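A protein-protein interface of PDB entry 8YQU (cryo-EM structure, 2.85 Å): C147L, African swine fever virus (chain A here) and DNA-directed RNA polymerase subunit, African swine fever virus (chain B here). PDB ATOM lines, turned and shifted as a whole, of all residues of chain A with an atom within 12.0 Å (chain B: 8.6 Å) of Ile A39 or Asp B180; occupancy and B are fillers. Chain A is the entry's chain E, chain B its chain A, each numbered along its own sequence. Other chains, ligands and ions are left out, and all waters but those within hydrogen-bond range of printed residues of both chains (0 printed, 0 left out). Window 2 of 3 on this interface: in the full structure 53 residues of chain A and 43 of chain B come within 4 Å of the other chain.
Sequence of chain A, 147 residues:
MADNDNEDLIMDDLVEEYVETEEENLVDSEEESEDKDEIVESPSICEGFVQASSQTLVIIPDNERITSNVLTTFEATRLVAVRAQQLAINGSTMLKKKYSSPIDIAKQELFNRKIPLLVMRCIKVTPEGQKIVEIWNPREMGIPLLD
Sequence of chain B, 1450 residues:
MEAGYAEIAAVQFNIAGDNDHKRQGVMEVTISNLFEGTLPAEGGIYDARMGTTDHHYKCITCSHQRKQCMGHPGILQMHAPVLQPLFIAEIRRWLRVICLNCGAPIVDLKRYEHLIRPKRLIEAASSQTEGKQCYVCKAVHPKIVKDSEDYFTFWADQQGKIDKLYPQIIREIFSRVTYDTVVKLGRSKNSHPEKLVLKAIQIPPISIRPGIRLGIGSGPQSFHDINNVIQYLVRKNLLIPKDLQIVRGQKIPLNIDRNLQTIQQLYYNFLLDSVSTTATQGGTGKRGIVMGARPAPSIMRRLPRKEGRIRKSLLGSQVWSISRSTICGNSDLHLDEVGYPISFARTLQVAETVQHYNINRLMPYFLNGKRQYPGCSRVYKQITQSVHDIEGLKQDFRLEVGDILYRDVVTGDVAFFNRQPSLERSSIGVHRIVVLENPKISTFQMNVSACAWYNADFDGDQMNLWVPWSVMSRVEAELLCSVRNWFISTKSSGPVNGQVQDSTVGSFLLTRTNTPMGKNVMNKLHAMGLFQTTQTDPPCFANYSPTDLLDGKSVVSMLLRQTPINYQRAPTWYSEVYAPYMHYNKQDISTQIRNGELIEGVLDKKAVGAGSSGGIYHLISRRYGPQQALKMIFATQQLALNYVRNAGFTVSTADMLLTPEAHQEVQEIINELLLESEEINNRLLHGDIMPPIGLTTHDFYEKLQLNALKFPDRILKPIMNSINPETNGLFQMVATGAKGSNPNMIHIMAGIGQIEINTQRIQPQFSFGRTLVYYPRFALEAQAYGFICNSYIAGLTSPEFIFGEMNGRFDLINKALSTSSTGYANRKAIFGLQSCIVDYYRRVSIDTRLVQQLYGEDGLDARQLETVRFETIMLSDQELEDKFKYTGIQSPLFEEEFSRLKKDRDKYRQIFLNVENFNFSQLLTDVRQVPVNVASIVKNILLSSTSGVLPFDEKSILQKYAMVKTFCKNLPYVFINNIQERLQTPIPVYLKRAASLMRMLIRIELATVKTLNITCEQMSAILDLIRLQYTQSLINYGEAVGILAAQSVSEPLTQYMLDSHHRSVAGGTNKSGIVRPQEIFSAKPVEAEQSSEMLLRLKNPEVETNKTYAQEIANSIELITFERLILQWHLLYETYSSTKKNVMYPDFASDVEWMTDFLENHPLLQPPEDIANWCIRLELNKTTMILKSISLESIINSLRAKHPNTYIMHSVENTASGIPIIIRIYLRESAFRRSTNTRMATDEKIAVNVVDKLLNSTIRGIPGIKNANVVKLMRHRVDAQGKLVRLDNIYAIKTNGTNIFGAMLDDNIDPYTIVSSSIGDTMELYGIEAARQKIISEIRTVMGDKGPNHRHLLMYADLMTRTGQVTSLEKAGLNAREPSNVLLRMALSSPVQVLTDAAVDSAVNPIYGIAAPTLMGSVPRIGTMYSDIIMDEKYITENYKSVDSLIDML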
ATOM      1  N   ILE A  39     -28.211   8.191  11.148  1.00  0.00           N
ATOM      2  CA  ILE A  39     -27.368   9.378  11.079  1.00  0.00           C
ATOM      3  C   ILE A  39     -26.536   9.510  12.349  1.00  0.00           C
ATOM      4  O   ILE A  39     -27.080   9.665  13.442  1.00  0.00           O
ATOM      5  CB  ILE A  39     -28.207  10.647  10.846  1.00  0.00           C
ATOM      6  CG1 ILE A  39     -28.926  10.574   9.498  1.00  0.00           C
ATOM      7  CG2 ILE A  39     -27.331  11.887  10.921  1.00  0.00           C
ATOM      8  CD1 ILE A  39     -29.969  11.651   9.304  1.00  0.00           C
ATOM      9  N   VAL A  40     -25.216   9.450  12.200  1.00  0.00           N
ATOM     10  CA  VAL A  40     -24.309   9.618  13.331  1.00  0.00           C
ATOM     11  C   VAL A  40     -24.212  11.112  13.622  1.00  0.00           C
ATOM     12  O   VAL A  40     -23.693  11.882  12.810  1.00  0.00           O
ATOM     13  CB  VAL A  40     -22.931   9.013  13.048  1.00  0.00           C
ATOM     14  CG1 VAL A  40     -21.997   9.285  14.210  1.00  0.00           C
ATOM     15  CG2 VAL A  40     -23.051   7.518  12.792  1.00  0.00           C
ATOM     16  N   GLU A  41     -24.710  11.520  14.781  1.00  0.00           N
ATOM     17  CA  GLU A  41     -24.976  12.915  15.082  1.00  0.00           C
ATOM     18  C   GLU A  41     -23.836  13.543  15.884  1.00  0.00           C
ATOM     19  O   GLU A  41     -22.759  12.964  16.046  1.00  0.00           O
ATOM     20  CB  GLU A  41     -26.313  13.018  15.811  1.00  0.00           C
ATOM     21  CG  GLU A  41     -27.485  12.649  14.931  1.00  0.00           C
ATOM     22  CD  GLU A  41     -28.801  12.717  15.660  1.00  0.00           C
ATOM     23  OE1 GLU A  41     -28.785  12.927  16.892  1.00  0.00           O
ATOM     24  OE2 GLU A  41     -29.848  12.556  15.000  1.00  0.00           O
ATOM     25  N   SER A  42     -24.086  14.749  16.388  1.00  0.00           N
ATOM     26  CA  SER A  42     -23.072  15.512  17.094  1.00  0.00           C
ATOM     27  C   SER A  42     -22.692  14.822  18.405  1.00  0.00           C
ATOM     28  O   SER A  42     -23.490  14.073  18.975  1.00  0.00           O
ATOM     29  CB  SER A  42     -23.582  16.922  17.376  1.00  0.00           C
ATOM     30  OG  SER A  42     -23.818  17.627  16.169  1.00  0.00           O
ATOM     31  N   PRO A  43     -21.472  15.050  18.896  1.00  0.00           N
ATOM     32  CA  PRO A  43     -21.049  14.406  20.145  1.00  0.00           C
ATOM     33  C   PRO A  43     -21.927  14.816  21.319  1.00  0.00           C
ATOM     34  O   PRO A  43     -22.389  15.956  21.409  1.00  0.00           O
ATOM     35  CB  PRO A  43     -19.606  14.891  20.327  1.00  0.00           C
ATOM     36  CG  PRO A  43     -19.487  16.105  19.465  1.00  0.00           C
ATOM     37  CD  PRO A  43     -20.402  15.872  18.307  1.00  0.00           C
ATOM     38  N   SER A  44     -22.151  13.869  22.223  1.00  0.00           N
ATOM     39  CA  SER A  44     -22.972  14.067  23.405  1.00  0.00           C
ATOM     40  C   SER A  44     -22.101  13.996  24.657  1.00  0.00           C
ATOM     41  O   SER A  44     -20.872  13.876  24.585  1.00  0.00           O
ATOM     42  CB  SER A  44     -24.100  13.034  23.438  1.00  0.00           C
ATOM     43  OG  SER A  44     -23.583  11.715  23.431  1.00  0.00           O
ATOM     44  N   GLU A  47     -20.521  10.196  25.748  1.00  0.00           N
ATOM     45  CA  GLU A  47     -19.169   9.969  25.270  1.00  0.00           C
ATOM     46  C   GLU A  47     -18.294  11.184  25.569  1.00  0.00           C
ATOM     47  O   GLU A  47     -18.780  12.285  25.836  1.00  0.00           O
ATOM     48  CB  GLU A  47     -19.178   9.661  23.773  1.00  0.00           C
ATOM     49  CG  GLU A  47     -19.653  10.815  22.908  1.00  0.00           C
ATOM     50  CD  GLU A  47     -19.719  10.452  21.439  1.00  0.00           C
ATOM     51  OE1 GLU A  47     -19.411   9.291  21.096  1.00  0.00           O
ATOM     52  OE2 GLU A  47     -20.084  11.326  20.626  1.00  0.00           O
ATOM     53  N   TRP B  94      -9.370  17.262   3.110  1.00  0.00           N
ATOM     54  CA  TRP B  94     -10.739  17.712   3.310  1.00  0.00           C
ATOM     55  C   TRP B  94     -11.204  18.645   2.204  1.00  0.00           C
ATOM     56  O   TRP B  94     -12.413  18.821   2.031  1.00  0.00           O
ATOM     57  CB  TRP B  94     -10.880  18.392   4.671  1.00  0.00           C
ATOM     58  CG  TRP B  94     -10.955  17.426   5.807  1.00  0.00           C
ATOM     59  CD1 TRP B  94     -10.023  17.236   6.784  1.00  0.00           C
ATOM     60  CD2 TRP B  94     -12.015  16.501   6.078  1.00  0.00           C
ATOM     61  NE1 TRP B  94     -10.441  16.257   7.652  1.00  0.00           N
ATOM     62  CE2 TRP B  94     -11.661  15.789   7.239  1.00  0.00           C
ATOM     63  CE3 TRP B  94     -13.232  16.210   5.454  1.00  0.00           C
ATOM     64  CZ2 TRP B  94     -12.477  14.805   7.788  1.00  0.00           C
ATOM     65  CZ3 TRP B  94     -14.041  15.233   6.001  1.00  0.00           C
ATOM     66  CH2 TRP B  94     -13.661  14.542   7.156  1.00  0.00           C
ATOM     67  N   PRO B 105     -20.539  15.450   1.020  1.00  0.00           N
ATOM     68  CA  PRO B 105     -19.466  14.674   0.389  1.00  0.00           C
ATOM     69  C   PRO B 105     -19.747  14.467  -1.089  1.00  0.00           C
ATOM     70  O   PRO B 105     -20.896  14.316  -1.509  1.00  0.00           O
ATOM     71  CB  PRO B 105     -19.483  13.350   1.159  1.00  0.00           C
ATOM     72  CG  PRO B 105     -20.887  13.217   1.626  1.00  0.00           C
ATOM     73  CD  PRO B 105     -21.358  14.620   1.920  1.00  0.00           C
ATOM     74  N   LEU B 109     -19.692   7.690   0.191  1.00  0.00           N
ATOM     75  CA  LEU B 109     -19.111   7.215   1.443  1.00  0.00           C
ATOM     76  C   LEU B 109     -19.185   5.696   1.547  1.00  0.00           C
ATOM     77  O   LEU B 109     -18.252   5.057   2.048  1.00  0.00           O
ATOM     78  CB  LEU B 109     -19.816   7.874   2.629  1.00  0.00           C
ATOM     79  CG  LEU B 109     -19.748   9.402   2.685  1.00  0.00           C
ATOM     80  CD1 LEU B 109     -20.296   9.917   4.006  1.00  0.00           C
ATOM     81  CD2 LEU B 109     -18.325   9.893   2.465  1.00  0.00           C
ATOM     82  N   ARG B 120      -9.536   5.576   5.217  1.00  0.00           N
ATOM     83  CA  ARG B 120     -10.725   5.919   4.443  1.00  0.00           C
ATOM     84  C   ARG B 120     -10.559   7.259   3.738  1.00  0.00           C
ATOM     85  O   ARG B 120     -10.754   7.363   2.522  1.00  0.00           O
ATOM     86  CB  ARG B 120     -11.957   5.940   5.348  1.00  0.00           C
ATOM     87  CG  ARG B 120     -12.486   4.568   5.728  1.00  0.00           C
ATOM     88  CD  ARG B 120     -13.797   4.684   6.487  1.00  0.00           C
ATOM     89  NE  ARG B 120     -14.238   3.401   7.022  1.00  0.00           N
ATOM     90  CZ  ARG B 120     -15.305   3.239   7.793  1.00  0.00           C
ATOM     91  NH1 ARG B 120     -16.072   4.260   8.136  1.00  0.00           N
ATOM     92  NH2 ARG B 120     -15.610   2.021   8.232  1.00  0.00           N
ATOM     93  N   VAL B 177     -19.548  21.233   7.186  1.00  0.00           N
ATOM     94  CA  VAL B 177     -19.476  19.784   7.113  1.00  0.00           C
ATOM     95  C   VAL B 177     -20.076  19.190   8.379  1.00  0.00           C
ATOM     96  O   VAL B 177     -19.771  19.631   9.493  1.00  0.00           O
ATOM     97  CB  VAL B 177     -18.024  19.337   6.909  1.00  0.00           C
ATOM     98  CG1 VAL B 177     -17.901  17.809   6.826  1.00  0.00           C
ATOM     99  CG2 VAL B 177     -17.475  19.995   5.666  1.00  0.00           C
ATOM    100  N   THR B 178     -20.955  18.206   8.202  1.00  0.00           N
ATOM    101  CA  THR B 178     -21.626  17.554   9.313  1.00  0.00           C
ATOM    102  C   THR B 178     -20.748  16.465   9.924  1.00  0.00           C
ATOM    103  O   THR B 178     -19.860  15.906   9.277  1.00  0.00           O
ATOM    104  CB  THR B 178     -22.953  16.955   8.859  1.00  0.00           C
ATOM    105  OG1 THR B 178     -22.712  15.935   7.880  1.00  0.00           O
ATOM    106  CG2 THR B 178     -23.836  18.027   8.254  1.00  0.00           C
ATOM    107  N   TYR B 179     -21.016  16.169  11.200  1.00  0.00           N
ATOM    108  CA  TYR B 179     -20.289  15.112  11.896  1.00  0.00           C
ATOM    109  C   TYR B 179     -20.556  13.736  11.303  1.00  0.00           C
ATOM    110  O   TYR B 179     -19.721  12.838  11.456  1.00  0.00           O
ATOM    111  CB  TYR B 179     -20.649  15.109  13.385  1.00  0.00           C
ATOM    112  CG  TYR B 179     -19.930  16.162  14.194  1.00  0.00           C
ATOM    113  CD1 TYR B 179     -18.588  16.023  14.515  1.00  0.00           C
ATOM    114  CD2 TYR B 179     -20.593  17.301  14.629  1.00  0.00           C
ATOM    115  CE1 TYR B 179     -17.928  16.981  15.254  1.00  0.00           C
ATOM    116  CE2 TYR B 179     -19.940  18.268  15.365  1.00  0.00           C
ATOM    117  CZ  TYR B 179     -18.606  18.102  15.674  1.00  0.00           C
ATOM    118  OH  TYR B 179     -17.944  19.057  16.408  1.00  0.00           O
ATOM    119  N   ASP B 180     -21.699  13.549  10.640  1.00  0.00           N
ATOM    120  CA  ASP B 180     -21.969  12.276   9.980  1.00  0.00           C
ATOM    121  C   ASP B 180     -20.945  12.010   8.883  1.00  0.00           C
ATOM    122  O   ASP B 180     -20.445  10.887   8.744  1.00  0.00           O
ATOM    123  CB  ASP B 180     -23.390  12.280   9.411  1.00  0.00           C
ATOM    124  CG  ASP B 180     -23.833  10.915   8.922  1.00  0.00           C
ATOM    125  OD1 ASP B 180     -23.033   9.962   9.004  1.00  0.00           O
ATOM    126  OD2 ASP B 180     -24.986  10.795   8.454  1.00  0.00           O
ATOM    127  N   THR B 181     -20.614  13.040   8.100  1.00  0.00           N
ATOM    128  CA  THR B 181     -19.597  12.894   7.064  1.00  0.00           C
ATOM    129  C   THR B 181     -18.242  12.554   7.669  1.00  0.00           C
ATOM    130  O   THR B 181     -17.519  11.697   7.148  1.00  0.00           O
ATOM    131  CB  THR B 181     -19.509  14.175   6.234  1.00  0.00           C
ATOM    132  OG1 THR B 181     -20.757  14.401   5.568  1.00  0.00           O
ATOM    133  CG2 THR B 181     -18.401  14.069   5.198  1.00  0.00           C
ATOM    134  N   VAL B 182     -17.883  13.213   8.773  1.00  0.00           N
ATOM    135  CA  VAL B 182     -16.602  12.943   9.422  1.00  0.00           C
ATOM    136  C   VAL B 182     -16.550  11.508   9.927  1.00  0.00           C
ATOM    137  O   VAL B 182     -15.543  10.810   9.760  1.00  0.00           O
ATOM    138  CB  VAL B 182     -16.359  13.953  10.559  1.00  0.00           C
ATOM    139  CG1 VAL B 182     -15.040  13.665  11.253  1.00  0.00           C
ATOM    140  CG2 VAL B 182     -16.385  15.374  10.021  1.00  0.00           C
ATOM    141  N   VAL B 183     -17.633  11.043  10.553  1.00  0.00           N
ATOM    142  CA  VAL B 183     -17.639   9.703  11.133  1.00  0.00           C
ATOM    143  C   VAL B 183     -17.597   8.643  10.040  1.00  0.00           C
ATOM    144  O   VAL B 183     -16.820   7.683  10.115  1.00  0.00           O
ATOM    145  CB  VAL B 183     -18.859   9.523  12.052  1.00  0.00           C
ATOM    146  CG1 VAL B 183     -19.035   8.060  12.421  1.00  0.00           C
ATOM    147  CG2 VAL B 183     -18.698  10.372  13.303  1.00  0.00           C
ATOM    148  N   LYS B 184     -18.422   8.795   9.002  1.00  0.00           N
ATOM    149  CA  LYS B 184     -18.422   7.815   7.922  1.00  0.00           C
ATOM    150  C   LYS B 184     -17.182   7.892   7.043  1.00  0.00           C
ATOM    151  O   LYS B 184     -16.980   6.999   6.213  1.00  0.00           O
ATOM    152  CB  LYS B 184     -19.676   7.962   7.057  1.00  0.00           C
ATOM    153  CG  LYS B 184     -20.962   7.550   7.754  1.00  0.00           C
ATOM    154  CD  LYS B 184     -22.156   7.672   6.822  1.00  0.00           C
ATOM    155  CE  LYS B 184     -23.446   7.261   7.513  1.00  0.00           C
ATOM    156  NZ  LYS B 184     -24.622   7.395   6.613  1.00  0.00           N
ATOM    157  N   LEU B 185     -16.352   8.922   7.196  1.00  0.00           N
ATOM    158  CA  LEU B 185     -15.077   9.002   6.498  1.00  0.00           C
ATOM    159  C   LEU B 185     -13.917   8.507   7.351  1.00  0.00           C
ATOM    160  O   LEU B 185     -12.758   8.659   6.951  1.00  0.00           O
ATOM    161  CB  LEU B 185     -14.812  10.433   6.031  1.00  0.00           C
ATOM    162  CG  LEU B 185     -15.354  10.780   4.644  1.00  0.00           C
ATOM    163  CD1 LEU B 185     -15.100  12.241   4.322  1.00  0.00           C
ATOM    164  CD2 LEU B 185     -14.733   9.880   3.589  1.00  0.00           C
ATOM    165  N   GLY B 186     -14.200   7.929   8.514  1.00  0.00           N
ATOM    166  CA  GLY B 186     -13.165   7.330   9.332  1.00  0.00           C
ATOM    167  C   GLY B 186     -12.700   8.184  10.493  1.00  0.00           C
ATOM    168  O   GLY B 186     -12.394   7.662  11.569  1.00  0.00           O
ATOM    169  N   ARG B 187     -12.639   9.496  10.289  1.00  0.00           N
ATOM    170  CA  ARG B 187     -12.140  10.391  11.321  1.00  0.00           C
ATOM    171  C   ARG B 187     -13.113  10.466  12.493  1.00  0.00           C
ATOM    172  O   ARG B 187     -14.330  10.352  12.330  1.00  0.00           O
ATOM    173  CB  ARG B 187     -11.900  11.784  10.744  1.00  0.00           C
ATOM    174  CG  ARG B 187     -10.798  11.828   9.702  1.00  0.00           C
ATOM    175  CD  ARG B 187      -9.426  11.806  10.350  1.00  0.00           C
ATOM    176  NE  ARG B 187      -8.356  11.816   9.361  1.00  0.00           N
ATOM    177  CZ  ARG B 187      -7.590  10.771   9.079  1.00  0.00           C
ATOM    178  NH1 ARG B 187      -7.747   9.612   9.696  1.00  0.00           N
ATOM    179  NH2 ARG B 187      -6.641  10.893   8.155  1.00  0.00           N
ATOM    180  N   LYS B 189     -14.968  12.202  15.954  1.00  0.00           N
ATOM    181  CA  LYS B 189     -15.649  13.471  16.185  1.00  0.00           C
ATOM    182  C   LYS B 189     -14.684  14.550  16.658  1.00  0.00           C
ATOM    183  O   LYS B 189     -14.922  15.740  16.426  1.00  0.00           O
ATOM    184  CB  LYS B 189     -16.776  13.285  17.199  1.00  0.00           C
ATOM    185  CG  LYS B 189     -17.893  12.376  16.721  1.00  0.00           C
ATOM    186  CD  LYS B 189     -19.036  12.348  17.719  1.00  0.00           C
ATOM    187  CE  LYS B 189     -20.086  11.329  17.322  1.00  0.00           C
ATOM    188  NZ  LYS B 189     -20.760  11.714  16.055  1.00  0.00           N
ATOM    189  N   HIS B 192     -12.734  16.846  13.650  1.00  0.00           N
ATOM    190  CA  HIS B 192     -13.536  17.593  12.694  1.00  0.00           C
ATOM    191  C   HIS B 192     -12.657  18.606  11.963  1.00  0.00           C
ATOM    192  O   HIS B 192     -11.780  19.224  12.575  1.00  0.00           O
ATOM    193  CB  HIS B 192     -14.686  18.306  13.404  1.00  0.00           C
ATOM    194  CG  HIS B 192     -15.772  18.772  12.486  1.00  0.00           C
ATOM    195  ND1 HIS B 192     -15.647  19.887  11.687  1.00  0.00           N
ATOM    196  CD2 HIS B 192     -17.007  18.272  12.242  1.00  0.00           C
ATOM    197  CE1 HIS B 192     -16.756  20.054  10.989  1.00  0.00           C
ATOM    198  NE2 HIS B 192     -17.598  19.087  11.308  1.00  0.00           N
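Printed residues of chain A within 4 Å of Asp B180: Ile A39 and Val A40. No residue of chain A comes within 4 Å of Thr B178. No residue of chain A comes within 4 Å of Thr B181. No residue of chain A comes within 4 Å of Val B182. No residue of chain A comes within 4 Å of Lys B184. Printed residues of chain A within 4 Å of Lys B189: Val A40 (3.3 Å), Glu A41 (2.4 Å), Pro A43 (3.7 Å) and Glu A47 (3.3 Å). Of the printed residues of chain B, Val A40 touches Tyr B179, Asp B180, Val B183 and Lys B189. Printed residues of chain B within 4 Å of Glu A47: Lys B189. Printed residues of chain A within 4 Å of Tyr B179: Val A40 (3.9 Å), Ser A42 (3.6 Å) and Pro A43 (3.8 Å). Arg B120 touches none of the printed residues of chain A. Trp B94 touches none of the printed residues of chain A. The nearest printed residue of chain B that does not touch Glu A41 is Tyr B179 (4.02 Å).
Among the printed residues, pairs that only touch across the chains: Glu A47 with Lys B189 (3.3 Å), Val A40 with Lys B189 (3.3 Å), Ile A39 with Asp B180 (3.6 Å), Ser A42 with Tyr B179 (3.6 Å), Val A40 with Val B183 (3.6 Å), Pro A43 with Lys B189 (3.7 Å), Pro A43 with Tyr B179 (3.8 Å) and Val A40 with Tyr B179 (3.9 Å).
Printed residues of chain A that touch a printed residue of chain B: Ile A39, Val A40, Glu A41, Ser A42, Pro A43 and Glu A47. Of the 17 printed residues of chain B, 4 touch a printed residue of chain A. Printed residues of chain B that touch a printed residue of chain A: Tyr B179, Asp B180, Val B183 and Lys B189. Hydrophobic or aromatic side chains of chain B within 4 Å of the printed part of chain A: Tyr B179 and Val B183. Among the printed residues, no Asp or Glu carboxylate lies within 4 Å of a Lys or Arg side-chain nitrogen of the other chain.
N of Asp B180 lies close to O of Val A40. NZ of Lys B189 sits close to O of Glu A41 (2.4 Å).
The side-chain amino group of Lys B184 is in salt-bridge range of the side-chain carboxylate of Asp B180 (3.9 Å).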
